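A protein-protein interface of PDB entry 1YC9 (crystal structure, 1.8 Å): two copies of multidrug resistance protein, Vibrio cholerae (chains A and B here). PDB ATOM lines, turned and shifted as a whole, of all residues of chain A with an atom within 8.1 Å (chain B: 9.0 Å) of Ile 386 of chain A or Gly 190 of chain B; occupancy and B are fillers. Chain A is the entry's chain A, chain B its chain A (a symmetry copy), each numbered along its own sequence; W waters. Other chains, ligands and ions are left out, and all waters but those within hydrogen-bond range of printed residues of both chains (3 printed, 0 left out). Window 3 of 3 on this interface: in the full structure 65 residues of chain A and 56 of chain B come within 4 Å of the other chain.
Water W3 lies within hydrogen-bond range of OG of Ser 193 of chain B (2.5 Å) and OE1 of Gln 379 of chain A (2.8 Å).
Water W2 lies within hydrogen-bond range of the backbone carbonyl oxygen of Ala 404 of chain A (2.6 Å), the backbone carbonyl oxygen of Ala 380 of chain A (2.7 Å) and the side-chain amide nitrogen of Gln 194 of chain B (3.4 Å).
Water W1 bridges O of Ala 383 of chain A (3.0 Å) and O of Gly 190 of chain B (3.2 Å).
No position is printed for both chains.
Gln 379 of chain A touches Ser 193 of chain B.
CD of Gln 379 of chain A touches CB of Lys 196 of chain B (3.8 Å).
Gln 379 of chain A touches Ala 197 of chain B (CB to N, 3.7 Å).
CB of Ala 197 of chain B touches N of Ala 380 of chain A, at 3.6 Å.
N of Ala 383 of chain A touches CB of Ser 193 of chain B, 3.7 Å away.
Gln 194 of chain B touches Ala 383 of chain A (OE1 to CB, 3.6 Å).
CD1 of Ile 386 of chain A touches CG of Leu 189 of chain B, at 3.5 Å.
Gly 190 of chain B touches Ile 386 of chain A (N to CG2, 3.6 Å).
Leu 399 of chain B touches Asp 400 of chain A.
Ala 404 of chain A touches Gln 194 of chain B.
Ile 386 of chain A touches just these residues of chain B: Leu 189 and Gly 190.
Printed residues of chain A within 4 Å of Gly 190 of chain B: Ala 383 (3.8 Å) and Ile 386 (3.6 Å).
Of the printed residues of chain B, Ala 383 of chain A touches Gly 190, Ser 193 and Gln 194.
No residue of chain B comes within 4 Å of Ala 387 of chain A.
Of the printed residues of chain A, Gln 194 of chain B touches Ala 383 and Ala 404.
Printed residues of chain B within 4 Å of Gln 379 of chain A: Ser 193 (3.4 Å), Lys 196 (3.8 Å) and Ala 197 (3.7 Å).
Tyr 398 of chain B touches none of the printed residues of chain A.
The nearest residue of chain A that does not touch Gly 190 of chain B is Gln 382 of chain A (5.4 Å).
Of the 20 printed residues of chain A, 7 touch a printed residue of chain B.
Printed residues of chain A that touch a printed residue of chain B: Gln 379, Ala 380, Gln 382, Ala 383, Ile 386, Asp 400 and Ala 404.
Hydrophobic or aromatic side chains of chain A that line the printed part of chain B: Ala 380, Ala 383, Ile 386 and Ala 404.
Hydrophobic or aromatic side chains of chain B within 4 Å of the printed part of chain A: Leu 189, Ala 197 and Leu 399.
Along chain B the printed residues that touch a printed residue of chain A span positions 189 to 399.
The backbone carbonyl oxygen of Leu 189 of chain B lies within hydrogen-bond range of the side-chain hydroxyl of Ser 193 of chain B, 2.9 Å away.
The side-chain hydroxyl (OG1) of Thr 188 of chain B lies within hydrogen-bond range of the backbone NH (N) of Gly 190 of chain B, at 2.9 Å.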
ATOM      1  N   GLN A 379       2.475  18.492 -14.188  1.00  0.00           N
ATOM      2  CA  GLN A 379       2.218  17.204 -14.820  1.00  0.00           C
ATOM      3  C   GLN A 379       1.855  17.332 -16.275  1.00  0.00           C
ATOM      4  O   GLN A 379       2.262  16.509 -17.092  1.00  0.00           O
ATOM      5  CB  GLN A 379       1.145  16.428 -14.092  1.00  0.00           C
ATOM      6  CG  GLN A 379       1.449  16.187 -12.680  1.00  0.00           C
ATOM      7  CD  GLN A 379       2.426  15.082 -12.445  1.00  0.00           C
ATOM      8  OE1 GLN A 379       2.913  14.448 -13.386  1.00  0.00           O
ATOM      9  NE2 GLN A 379       2.656  14.788 -11.168  1.00  0.00           N
ATOM     10  N   ALA A 380       1.141  18.398 -16.632  1.00  0.00           N
ATOM     11  CA  ALA A 380       0.849  18.612 -18.027  1.00  0.00           C
ATOM     12  C   ALA A 380       2.132  18.961 -18.801  1.00  0.00           C
ATOM     13  O   ALA A 380       2.280  18.609 -19.986  1.00  0.00           O
ATOM     14  CB  ALA A 380      -0.233  19.751 -18.149  1.00  0.00           C
ATOM     15  N   GLU A 381       3.055  19.654 -18.141  1.00  0.00           N
ATOM     16  CA  GLU A 381       4.285  20.064 -18.780  1.00  0.00           C
ATOM     17  C   GLU A 381       5.127  18.809 -19.051  1.00  0.00           C
ATOM     18  O   GLU A 381       5.633  18.654 -20.142  1.00  0.00           O
ATOM     19  CB  GLU A 381       5.057  20.993 -17.895  1.00  0.00           C
ATOM     20  CG  GLU A 381       6.289  21.523 -18.554  1.00  0.00           C
ATOM     21  CD  GLU A 381       7.018  22.500 -17.685  1.00  0.00           C
ATOM     22  OE1 GLU A 381       6.417  22.943 -16.659  1.00  0.00           O
ATOM     23  OE2 GLU A 381       8.183  22.814 -18.039  1.00  0.00           O
ATOM     24  N   GLN A 382       5.192  17.916 -18.077  1.00  0.00           N
ATOM     25  CA  GLN A 382       5.810  16.596 -18.302  1.00  0.00           C
ATOM     26  C   GLN A 382       5.144  15.825 -19.425  1.00  0.00           C
ATOM     27  O   GLN A 382       5.808  15.261 -20.308  1.00  0.00           O
ATOM     28  CB  GLN A 382       5.795  15.755 -17.025  1.00  0.00           C
ATOM     29  CG  GLN A 382       6.664  14.482 -17.165  1.00  0.00           C
ATOM     30  N   ALA A 383       3.815  15.789 -19.430  1.00  0.00           N
ATOM     31  CA  ALA A 383       3.093  15.118 -20.480  1.00  0.00           C
ATOM     32  C   ALA A 383       3.467  15.623 -21.855  1.00  0.00           C
ATOM     33  O   ALA A 383       3.670  14.813 -22.751  1.00  0.00           O
ATOM     34  CB  ALA A 383       1.591  15.183 -20.265  1.00  0.00           C
ATOM     35  N   LEU A 384       3.603  16.928 -21.998  1.00  0.00           N
ATOM     36  CA  LEU A 384       3.899  17.550 -23.264  1.00  0.00           C
ATOM     37  C   LEU A 384       5.330  17.223 -23.670  1.00  0.00           C
ATOM     38  O   LEU A 384       5.575  16.966 -24.820  1.00  0.00           O
ATOM     39  CB  LEU A 384       3.790  19.062 -23.175  1.00  0.00           C
ATOM     40  CG  LEU A 384       4.140  19.826 -24.459  1.00  0.00           C
ATOM     41  CD1 LEU A 384       3.269  19.381 -25.608  1.00  0.00           C
ATOM     42  CD2 LEU A 384       4.004  21.302 -24.262  1.00  0.00           C
ATOM     43  N   HIS A 385       6.241  17.342 -22.719  1.00  0.00           N
ATOM     44  CA  HIS A 385       7.669  17.045 -22.935  1.00  0.00           C
ATOM     45  C   HIS A 385       7.813  15.619 -23.437  1.00  0.00           C
ATOM     46  O   HIS A 385       8.469  15.396 -24.446  1.00  0.00           O
ATOM     47  CB  HIS A 385       8.496  17.315 -21.654  1.00  0.00           C
ATOM     48  CG  HIS A 385       9.844  16.640 -21.645  1.00  0.00           C
ATOM     49  ND1 HIS A 385      11.027  17.330 -21.847  1.00  0.00           N
ATOM     50  CD2 HIS A 385      10.190  15.335 -21.484  1.00  0.00           C
ATOM     51  CE1 HIS A 385      12.043  16.479 -21.795  1.00  0.00           C
ATOM     52  NE2 HIS A 385      11.563  15.260 -21.588  1.00  0.00           N
ATOM     53  N   ILE A 386       7.156  14.651 -22.798  1.00  0.00           N
ATOM     54  CA  ILE A 386       7.212  13.280 -23.244  1.00  0.00           C
ATOM     55  C   ILE A 386       6.544  13.131 -24.606  1.00  0.00           C
ATOM     56  O   ILE A 386       7.044  12.413 -25.452  1.00  0.00           O
ATOM     57  CB  ILE A 386       6.592  12.317 -22.223  1.00  0.00           C
ATOM     58  CG1 ILE A 386       7.515  12.154 -21.025  1.00  0.00           C
ATOM     59  CG2 ILE A 386       6.333  10.983 -22.817  1.00  0.00           C
ATOM     60  CD1 ILE A 386       6.809  11.930 -19.746  1.00  0.00           C
ATOM     61  N   ALA A 387       5.407  13.805 -24.817  1.00  0.00           N
ATOM     62  CA  ALA A 387       4.686  13.666 -26.075  1.00  0.00           C
ATOM     63  C   ALA A 387       5.517  14.216 -27.226  1.00  0.00           C
ATOM     64  O   ALA A 387       5.496  13.642 -28.312  1.00  0.00           O
ATOM     65  CB  ALA A 387       3.315  14.402 -25.997  1.00  0.00           C
ATOM     66  N   THR A 388       6.234  15.310 -26.998  1.00  0.00           N
ATOM     67  CA  THR A 388       6.984  15.918 -28.084  1.00  0.00           C
ATOM     68  C   THR A 388       8.311  15.167 -28.343  1.00  0.00           C
ATOM     69  O   THR A 388       8.741  15.080 -29.485  1.00  0.00           O
ATOM     70  CB  THR A 388       7.292  17.405 -27.867  1.00  0.00           C
ATOM     71  OG1 THR A 388       8.126  17.587 -26.726  1.00  0.00           O
ATOM     72  CG2 THR A 388       6.010  18.252 -27.538  1.00  0.00           C
ATOM     73  N   ASN A 389       8.966  14.670 -27.286  1.00  0.00           N
ATOM     74  CA  ASN A 389      10.157  13.810 -27.458  1.00  0.00           C
ATOM     75  C   ASN A 389       9.781  12.616 -28.282  1.00  0.00           C
ATOM     76  O   ASN A 389      10.399  12.360 -29.323  1.00  0.00           O
ATOM     77  CB  ASN A 389      10.709  13.327 -26.119  1.00  0.00           C
ATOM     78  CG  ASN A 389      11.475  14.382 -25.390  1.00  0.00           C
ATOM     79  OD1 ASN A 389      12.011  15.301 -25.981  1.00  0.00           O
ATOM     80  ND2 ASN A 389      11.546  14.247 -24.062  1.00  0.00           N
ATOM     81  N   ARG A 390       8.727  11.922 -27.863  1.00  0.00           N
ATOM     82  CA  ARG A 390       8.189  10.795 -28.599  1.00  0.00           C
ATOM     83  C   ARG A 390       7.804  11.174 -30.032  1.00  0.00           C
ATOM     84  O   ARG A 390       7.927  10.355 -30.970  1.00  0.00           O
ATOM     85  CB  ARG A 390       6.973  10.174 -27.892  1.00  0.00           C
ATOM     86  CG  ARG A 390       7.313   9.229 -26.741  1.00  0.00           C
ATOM     87  CD  ARG A 390       6.116   8.779 -25.903  1.00  0.00           C
ATOM     88  NE  ARG A 390       5.368   7.657 -26.465  1.00  0.00           N
ATOM     89  CZ  ARG A 390       5.813   6.396 -26.558  1.00  0.00           C
ATOM     90  NH1 ARG A 390       7.038   6.047 -26.149  1.00  0.00           N
ATOM     91  NH2 ARG A 390       5.017   5.467 -27.074  1.00  0.00           N
ATOM     92  N   TYR A 391       7.303  12.394 -30.213  1.00  0.00           N
ATOM     93  CA  TYR A 391       6.965  12.833 -31.564  1.00  0.00           C
ATOM     94  C   TYR A 391       8.255  13.059 -32.384  1.00  0.00           C
ATOM     95  O   TYR A 391       8.384  12.587 -33.470  1.00  0.00           O
ATOM     96  CB  TYR A 391       6.071  14.089 -31.558  1.00  0.00           C
ATOM     97  CG  TYR A 391       5.575  14.414 -32.941  1.00  0.00           C
ATOM     98  CD1 TYR A 391       4.501  13.753 -33.481  1.00  0.00           C
ATOM     99  CD2 TYR A 391       6.235  15.344 -33.726  1.00  0.00           C
ATOM    100  CE1 TYR A 391       4.064  14.030 -34.789  1.00  0.00           C
ATOM    101  CE2 TYR A 391       5.817  15.618 -35.030  1.00  0.00           C
ATOM    102  CZ  TYR A 391       4.729  14.961 -35.552  1.00  0.00           C
ATOM    103  OH  TYR A 391       4.308  15.242 -36.849  1.00  0.00           O
ATOM    104  N   GLN A 392       9.223  13.773 -31.840  1.00  0.00           N
ATOM    105  CA  GLN A 392      10.469  14.023 -32.542  1.00  0.00           C
ATOM    106  C   GLN A 392      11.211  12.694 -32.843  1.00  0.00           C
ATOM    107  O   GLN A 392      12.270  12.723 -33.477  1.00  0.00           O
ATOM    108  CB  GLN A 392      11.358  14.989 -31.730  1.00  0.00           C
ATOM    109  CG  GLN A 392      10.814  16.440 -31.591  1.00  0.00           C
ATOM    110  CD  GLN A 392      11.771  17.407 -30.854  1.00  0.00           C
ATOM    111  OE1 GLN A 392      12.078  17.233 -29.667  1.00  0.00           O
ATOM    112  NE2 GLN A 392      12.216  18.440 -31.558  1.00  0.00           N
ATOM    113  N   GLY A 393      10.656  11.552 -32.402  1.00  0.00           N
ATOM    114  CA  GLY A 393      11.197  10.227 -32.653  1.00  0.00           C
ATOM    115  C   GLY A 393      10.205   9.179 -33.155  1.00  0.00           C
ATOM    116  O   GLY A 393      10.495   7.989 -33.124  1.00  0.00           O
ATOM    117  N   LEU A 395       7.060   7.800 -32.252  1.00  0.00           N
ATOM    118  CA  LEU A 395       6.369   6.813 -31.415  1.00  0.00           C
ATOM    119  C   LEU A 395       4.969   7.252 -30.986  1.00  0.00           C
ATOM    120  O   LEU A 395       4.109   6.415 -30.634  1.00  0.00           O
ATOM    121  CB  LEU A 395       7.204   6.557 -30.167  1.00  0.00           C
ATOM    122  CG  LEU A 395       8.190   5.389 -30.327  1.00  0.00           C
ATOM    123  CD1 LEU A 395       9.434   5.633 -29.460  1.00  0.00           C
ATOM    124  CD2 LEU A 395       7.473   4.062 -29.995  1.00  0.00           C
ATOM    125  N   ALA A 396       4.746   8.566 -30.978  1.00  0.00           N
ATOM    126  CA  ALA A 396       3.440   9.126 -30.652  1.00  0.00           C
ATOM    127  C   ALA A 396       2.922   9.997 -31.790  1.00  0.00           C
ATOM    128  O   ALA A 396       3.704  10.541 -32.574  1.00  0.00           O
ATOM    129  CB  ALA A 396       3.546   9.956 -29.405  1.00  0.00           C
ATOM    130  N   ASP A 400      -1.409  13.469 -29.569  1.00  0.00           N
ATOM    131  CA  ASP A 400      -0.941  13.441 -28.187  1.00  0.00           C
ATOM    132  C   ASP A 400      -0.322  14.753 -27.811  1.00  0.00           C
ATOM    133  O   ASP A 400      -0.498  15.236 -26.692  1.00  0.00           O
ATOM    134  CB  ASP A 400       0.034  12.301 -27.934  1.00  0.00           C
ATOM    135  CG  ASP A 400      -0.543  10.982 -28.281  1.00  0.00           C
ATOM    136  OD1 ASP A 400      -1.723  10.701 -27.957  1.00  0.00           O
ATOM    137  OD2 ASP A 400       0.115  10.138 -28.911  1.00  0.00           O
ATOM    138  N   VAL A 401       0.416  15.337 -28.753  1.00  0.00           N
ATOM    139  CA  VAL A 401       1.016  16.623 -28.567  1.00  0.00           C
ATOM    140  C   VAL A 401      -0.067  17.720 -28.421  1.00  0.00           C
ATOM    141  O   VAL A 401      -0.003  18.524 -27.507  1.00  0.00           O
ATOM    142  CB  VAL A 401       1.981  16.957 -29.685  1.00  0.00           C
ATOM    143  CG1 VAL A 401       2.425  18.358 -29.563  1.00  0.00           C
ATOM    144  CG2 VAL A 401       3.213  15.973 -29.644  1.00  0.00           C
ATOM    145  N   ALA A 404      -1.815  17.520 -24.979  1.00  0.00           N
ATOM    146  CA  ALA A 404      -0.939  17.984 -23.943  1.00  0.00           C
ATOM    147  C   ALA A 404      -0.701  19.489 -23.968  1.00  0.00           C
ATOM    148  O   ALA A 404      -0.665  20.119 -22.945  1.00  0.00           O
ATOM    149  CB  ALA A 404       0.412  17.214 -24.017  1.00  0.00           C
ATOM    150  N   LEU B 178      -3.020   3.364 -14.491  1.00  0.00           N
ATOM    151  CA  LEU B 178      -2.015   3.690 -15.494  1.00  0.00           C
ATOM    152  C   LEU B 178      -0.615   3.581 -14.914  1.00  0.00           C
ATOM    153  O   LEU B 178       0.304   3.257 -15.628  1.00  0.00           O
ATOM    154  CB  LEU B 178      -2.205   5.094 -16.073  1.00  0.00           C
ATOM    155  CG  LEU B 178      -3.001   5.209 -17.378  1.00  0.00           C
ATOM    156  CD1 LEU B 178      -4.392   4.584 -17.235  1.00  0.00           C
ATOM    157  CD2 LEU B 178      -3.101   6.667 -17.810  1.00  0.00           C
ATOM    158  N   TYR B 182       2.180   1.260 -16.343  1.00  0.00           N
ATOM    159  CA  TYR B 182       3.453   1.835 -16.710  1.00  0.00           C
ATOM    160  C   TYR B 182       4.595   1.064 -15.986  1.00  0.00           C
ATOM    161  O   TYR B 182       5.629   0.789 -16.577  1.00  0.00           O
ATOM    162  CB  TYR B 182       3.457   3.310 -16.345  1.00  0.00           C
ATOM    163  CG  TYR B 182       4.785   3.955 -16.378  1.00  0.00           C
ATOM    164  CD1 TYR B 182       5.432   4.181 -17.577  1.00  0.00           C
ATOM    165  CD2 TYR B 182       5.418   4.351 -15.197  1.00  0.00           C
ATOM    166  CE1 TYR B 182       6.659   4.795 -17.620  1.00  0.00           C
ATOM    167  CE2 TYR B 182       6.670   4.962 -15.236  1.00  0.00           C
ATOM    168  CZ  TYR B 182       7.267   5.175 -16.439  1.00  0.00           C
ATOM    169  OH  TYR B 182       8.492   5.762 -16.531  1.00  0.00           O
ATOM    170  N   GLU B 187       2.346   0.752 -20.347  1.00  0.00           N
ATOM    171  CA  GLU B 187       1.897   2.133 -20.626  1.00  0.00           C
ATOM    172  C   GLU B 187       3.100   3.109 -20.596  1.00  0.00           C
ATOM    173  O   GLU B 187       4.136   2.785 -20.011  1.00  0.00           O
ATOM    174  CB  GLU B 187       0.807   2.488 -19.594  1.00  0.00           C
ATOM    175  CG  GLU B 187       0.166   3.860 -19.740  1.00  0.00           C
ATOM    176  CD  GLU B 187      -0.484   4.061 -21.075  1.00  0.00           C
ATOM    177  OE1 GLU B 187       0.138   4.724 -21.943  1.00  0.00           O
ATOM    178  OE2 GLU B 187      -1.659   3.598 -21.215  1.00  0.00           O
ATOM    179  N   THR B 188       2.932   4.276 -21.209  1.00  0.00           N
ATOM    180  CA  THR B 188       3.973   5.293 -21.231  1.00  0.00           C
ATOM    181  C   THR B 188       3.876   6.228 -20.029  1.00  0.00           C
ATOM    182  O   THR B 188       2.862   6.271 -19.334  1.00  0.00           O
ATOM    183  CB  THR B 188       3.909   6.104 -22.539  1.00  0.00           C
ATOM    184  OG1 THR B 188       4.520   7.384 -22.341  1.00  0.00           O
ATOM    185  CG2 THR B 188       2.468   6.452 -22.880  1.00  0.00           C
ATOM    186  N   LEU B 189       4.951   6.974 -19.799  1.00  0.00           N
ATOM    187  CA  LEU B 189       5.013   7.977 -18.729  1.00  0.00           C
ATOM    188  C   LEU B 189       4.159   9.220 -19.107  1.00  0.00           C
ATOM    189  O   LEU B 189       3.628   9.894 -18.241  1.00  0.00           O
ATOM    190  CB  LEU B 189       6.463   8.401 -18.482  1.00  0.00           C
ATOM    191  CG  LEU B 189       6.707   9.363 -17.325  1.00  0.00           C
ATOM    192  CD1 LEU B 189       6.111   8.923 -15.980  1.00  0.00           C
ATOM    193  CD2 LEU B 189       8.192   9.595 -17.147  1.00  0.00           C
ATOM    194  N   GLY B 190       4.080   9.497 -20.401  1.00  0.00           N
ATOM    195  CA  GLY B 190       3.242  10.556 -20.955  1.00  0.00           C
ATOM    196  C   GLY B 190       1.800  10.423 -20.544  1.00  0.00           C
ATOM    197  O   GLY B 190       1.205  11.385 -20.079  1.00  0.00           O
ATOM    198  N   SER B 191       1.261   9.221 -20.666  1.00  0.00           N
ATOM    199  CA  SER B 191      -0.093   8.911 -20.277  1.00  0.00           C
ATOM    200  C   SER B 191      -0.288   9.096 -18.807  1.00  0.00           C
ATOM    201  O   SER B 191      -1.269   9.688 -18.383  1.00  0.00           O
ATOM    202  CB  SER B 191      -0.462   7.479 -20.664  1.00  0.00           C
ATOM    203  OG  SER B 191      -0.429   7.373 -22.070  1.00  0.00           O
ATOM    204  N   VAL B 192       0.670   8.614 -18.034  1.00  0.00           N
ATOM    205  CA  VAL B 192       0.622   8.701 -16.598  1.00  0.00           C
ATOM    206  C   VAL B 192       0.616  10.190 -16.200  1.00  0.00           C
ATOM    207  O   VAL B 192      -0.176  10.596 -15.360  1.00  0.00           O
ATOM    208  CB  VAL B 192       1.848   7.983 -15.960  1.00  0.00           C
ATOM    209  CG1 VAL B 192       1.944   8.258 -14.451  1.00  0.00           C
ATOM    210  CG2 VAL B 192       1.790   6.466 -16.246  1.00  0.00           C
ATOM    211  N   SER B 193       1.458  10.980 -16.845  1.00  0.00           N
ATOM    212  CA  SER B 193       1.623  12.375 -16.468  1.00  0.00           C
ATOM    213  C   SER B 193       0.334  13.153 -16.821  1.00  0.00           C
ATOM    214  O   SER B 193      -0.114  13.988 -16.059  1.00  0.00           O
ATOM    215  CB  SER B 193       2.822  13.002 -17.155  1.00  0.00           C
ATOM    216  OG  SER B 193       4.033  12.381 -16.720  1.00  0.00           O
ATOM    217  N   GLN B 194      -0.252  12.818 -17.952  1.00  0.00           N
ATOM    218  CA  GLN B 194      -1.482  13.450 -18.412  1.00  0.00           C
ATOM    219  C   GLN B 194      -2.598  13.163 -17.448  1.00  0.00           C
ATOM    220  O   GLN B 194      -3.343  14.090 -17.077  1.00  0.00           O
ATOM    221  CB  GLN B 194      -1.830  12.979 -19.810  1.00  0.00           C
ATOM    222  CG  GLN B 194      -2.867  13.858 -20.516  1.00  0.00           C
ATOM    223  CD  GLN B 194      -2.338  15.214 -20.855  1.00  0.00           C
ATOM    224  OE1 GLN B 194      -1.668  15.368 -21.839  1.00  0.00           O
ATOM    225  NE2 GLN B 194      -2.629  16.208 -20.011  1.00  0.00           N
ATOM    226  N   ALA B 195      -2.674  11.928 -16.988  1.00  0.00           N
ATOM    227  CA  ALA B 195      -3.716  11.492 -16.086  1.00  0.00           C
ATOM    228  C   ALA B 195      -3.597  12.156 -14.749  1.00  0.00           C
ATOM    229  O   ALA B 195      -4.609  12.480 -14.097  1.00  0.00           O
ATOM    230  CB  ALA B 195      -3.721   9.991 -15.941  1.00  0.00           C
ATOM    231  N   LYS B 196      -2.353  12.345 -14.304  1.00  0.00           N
ATOM    232  CA  LYS B 196      -2.115  13.058 -13.068  1.00  0.00           C
ATOM    233  C   LYS B 196      -2.479  14.552 -13.217  1.00  0.00           C
ATOM    234  O   LYS B 196      -3.009  15.130 -12.290  1.00  0.00           O
ATOM    235  CB  LYS B 196      -0.670  12.871 -12.626  1.00  0.00           C
ATOM    236  CG  LYS B 196      -0.391  11.465 -12.189  1.00  0.00           C
ATOM    237  CD  LYS B 196       1.128  11.269 -11.912  1.00  0.00           C
ATOM    238  CE  LYS B 196       1.366   9.963 -11.189  1.00  0.00           C
ATOM    239  NZ  LYS B 196       1.014  10.086  -9.759  1.00  0.00           N
ATOM    240  N   ALA B 197      -2.256  15.115 -14.395  1.00  0.00           N
ATOM    241  CA  ALA B 197      -2.579  16.506 -14.673  1.00  0.00           C
ATOM    242  C   ALA B 197      -4.121  16.665 -14.651  1.00  0.00           C
ATOM    243  O   ALA B 197      -4.657  17.568 -13.955  1.00  0.00           O
ATOM    244  CB  ALA B 197      -2.035  16.919 -15.980  1.00  0.00           C
ATOM    245  N   VAL B 198      -4.799  15.723 -15.295  1.00  0.00           N
ATOM    246  CA  VAL B 198      -6.270  15.677 -15.273  1.00  0.00           C
ATOM    247  C   VAL B 198      -6.788  15.613 -13.834  1.00  0.00           C
ATOM    248  O   VAL B 198      -7.667  16.417 -13.455  1.00  0.00           O
ATOM    249  CB  VAL B 198      -6.831  14.506 -16.137  1.00  0.00           C
ATOM    250  CG1 VAL B 198      -8.353  14.295 -15.899  1.00  0.00           C
ATOM    251  CG2 VAL B 198      -6.597  14.770 -17.591  1.00  0.00           C
ATOM    252  N   TYR B 398      -5.134   5.402 -23.815  1.00  0.00           N
ATOM    253  CA  TYR B 398      -5.519   6.243 -22.697  1.00  0.00           C
ATOM    254  C   TYR B 398      -6.276   7.462 -23.252  1.00  0.00           C
ATOM    255  O   TYR B 398      -7.240   7.891 -22.665  1.00  0.00           O
ATOM    256  CB  TYR B 398      -4.293   6.717 -21.892  1.00  0.00           C
ATOM    257  CG  TYR B 398      -4.663   7.845 -20.947  1.00  0.00           C
ATOM    258  CD1 TYR B 398      -5.619   7.646 -19.951  1.00  0.00           C
ATOM    259  CD2 TYR B 398      -4.114   9.102 -21.094  1.00  0.00           C
ATOM    260  CE1 TYR B 398      -6.013   8.693 -19.106  1.00  0.00           C
ATOM    261  CE2 TYR B 398      -4.484  10.152 -20.257  1.00  0.00           C
ATOM    262  CZ  TYR B 398      -5.430   9.943 -19.272  1.00  0.00           C
ATOM    263  OH  TYR B 398      -5.793  10.996 -18.447  1.00  0.00           O
ATOM    264  N   LEU B 399      -5.828   7.999 -24.372  1.00  0.00           N
ATOM    265  CA  LEU B 399      -6.464   9.152 -24.977  1.00  0.00           C
ATOM    266  C   LEU B 399      -7.974   8.967 -25.169  1.00  0.00           C
ATOM    267  O   LEU B 399      -8.746   9.896 -24.939  1.00  0.00           O
ATOM    268  CB  LEU B 399      -5.886   9.436 -26.337  1.00  0.00           C
ATOM    269  CG  LEU B 399      -5.407  10.841 -26.644  1.00  0.00           C
ATOM    270  CD1 LEU B 399      -5.714  11.141 -28.078  1.00  0.00           C
ATOM    271  CD2 LEU B 399      -5.970  11.923 -25.708  1.00  0.00           C
ATOM    272  N   LEU B 402      -9.406   9.523 -21.808  1.00  0.00           N
ATOM    273  CA  LEU B 402      -9.386  10.929 -21.403  1.00  0.00           C
ATOM    274  C   LEU B 402     -10.518  11.714 -22.063  1.00  0.00           C
ATOM    275  O   LEU B 402     -11.170  12.495 -21.403  1.00  0.00           O
ATOM    276  CB  LEU B 402      -8.044  11.517 -21.760  1.00  0.00           C
ATOM    277  CG  LEU B 402      -7.775  13.004 -21.562  1.00  0.00           C
ATOM    278  CD1 LEU B 402      -6.303  13.219 -21.252  1.00  0.00           C
ATOM    279  CD2 LEU B 402      -8.144  13.785 -22.792  1.00  0.00           C
HETATM  280  O   HOH W   1       2.025  12.345 -23.042  1.00  0.00           O
HETATM  281  O   HOH W   2      -0.240  18.371 -21.042  1.00  0.00           O
HETATM  282  O   HOH W   3       4.337  12.189 -14.281  1.00  0.00           O
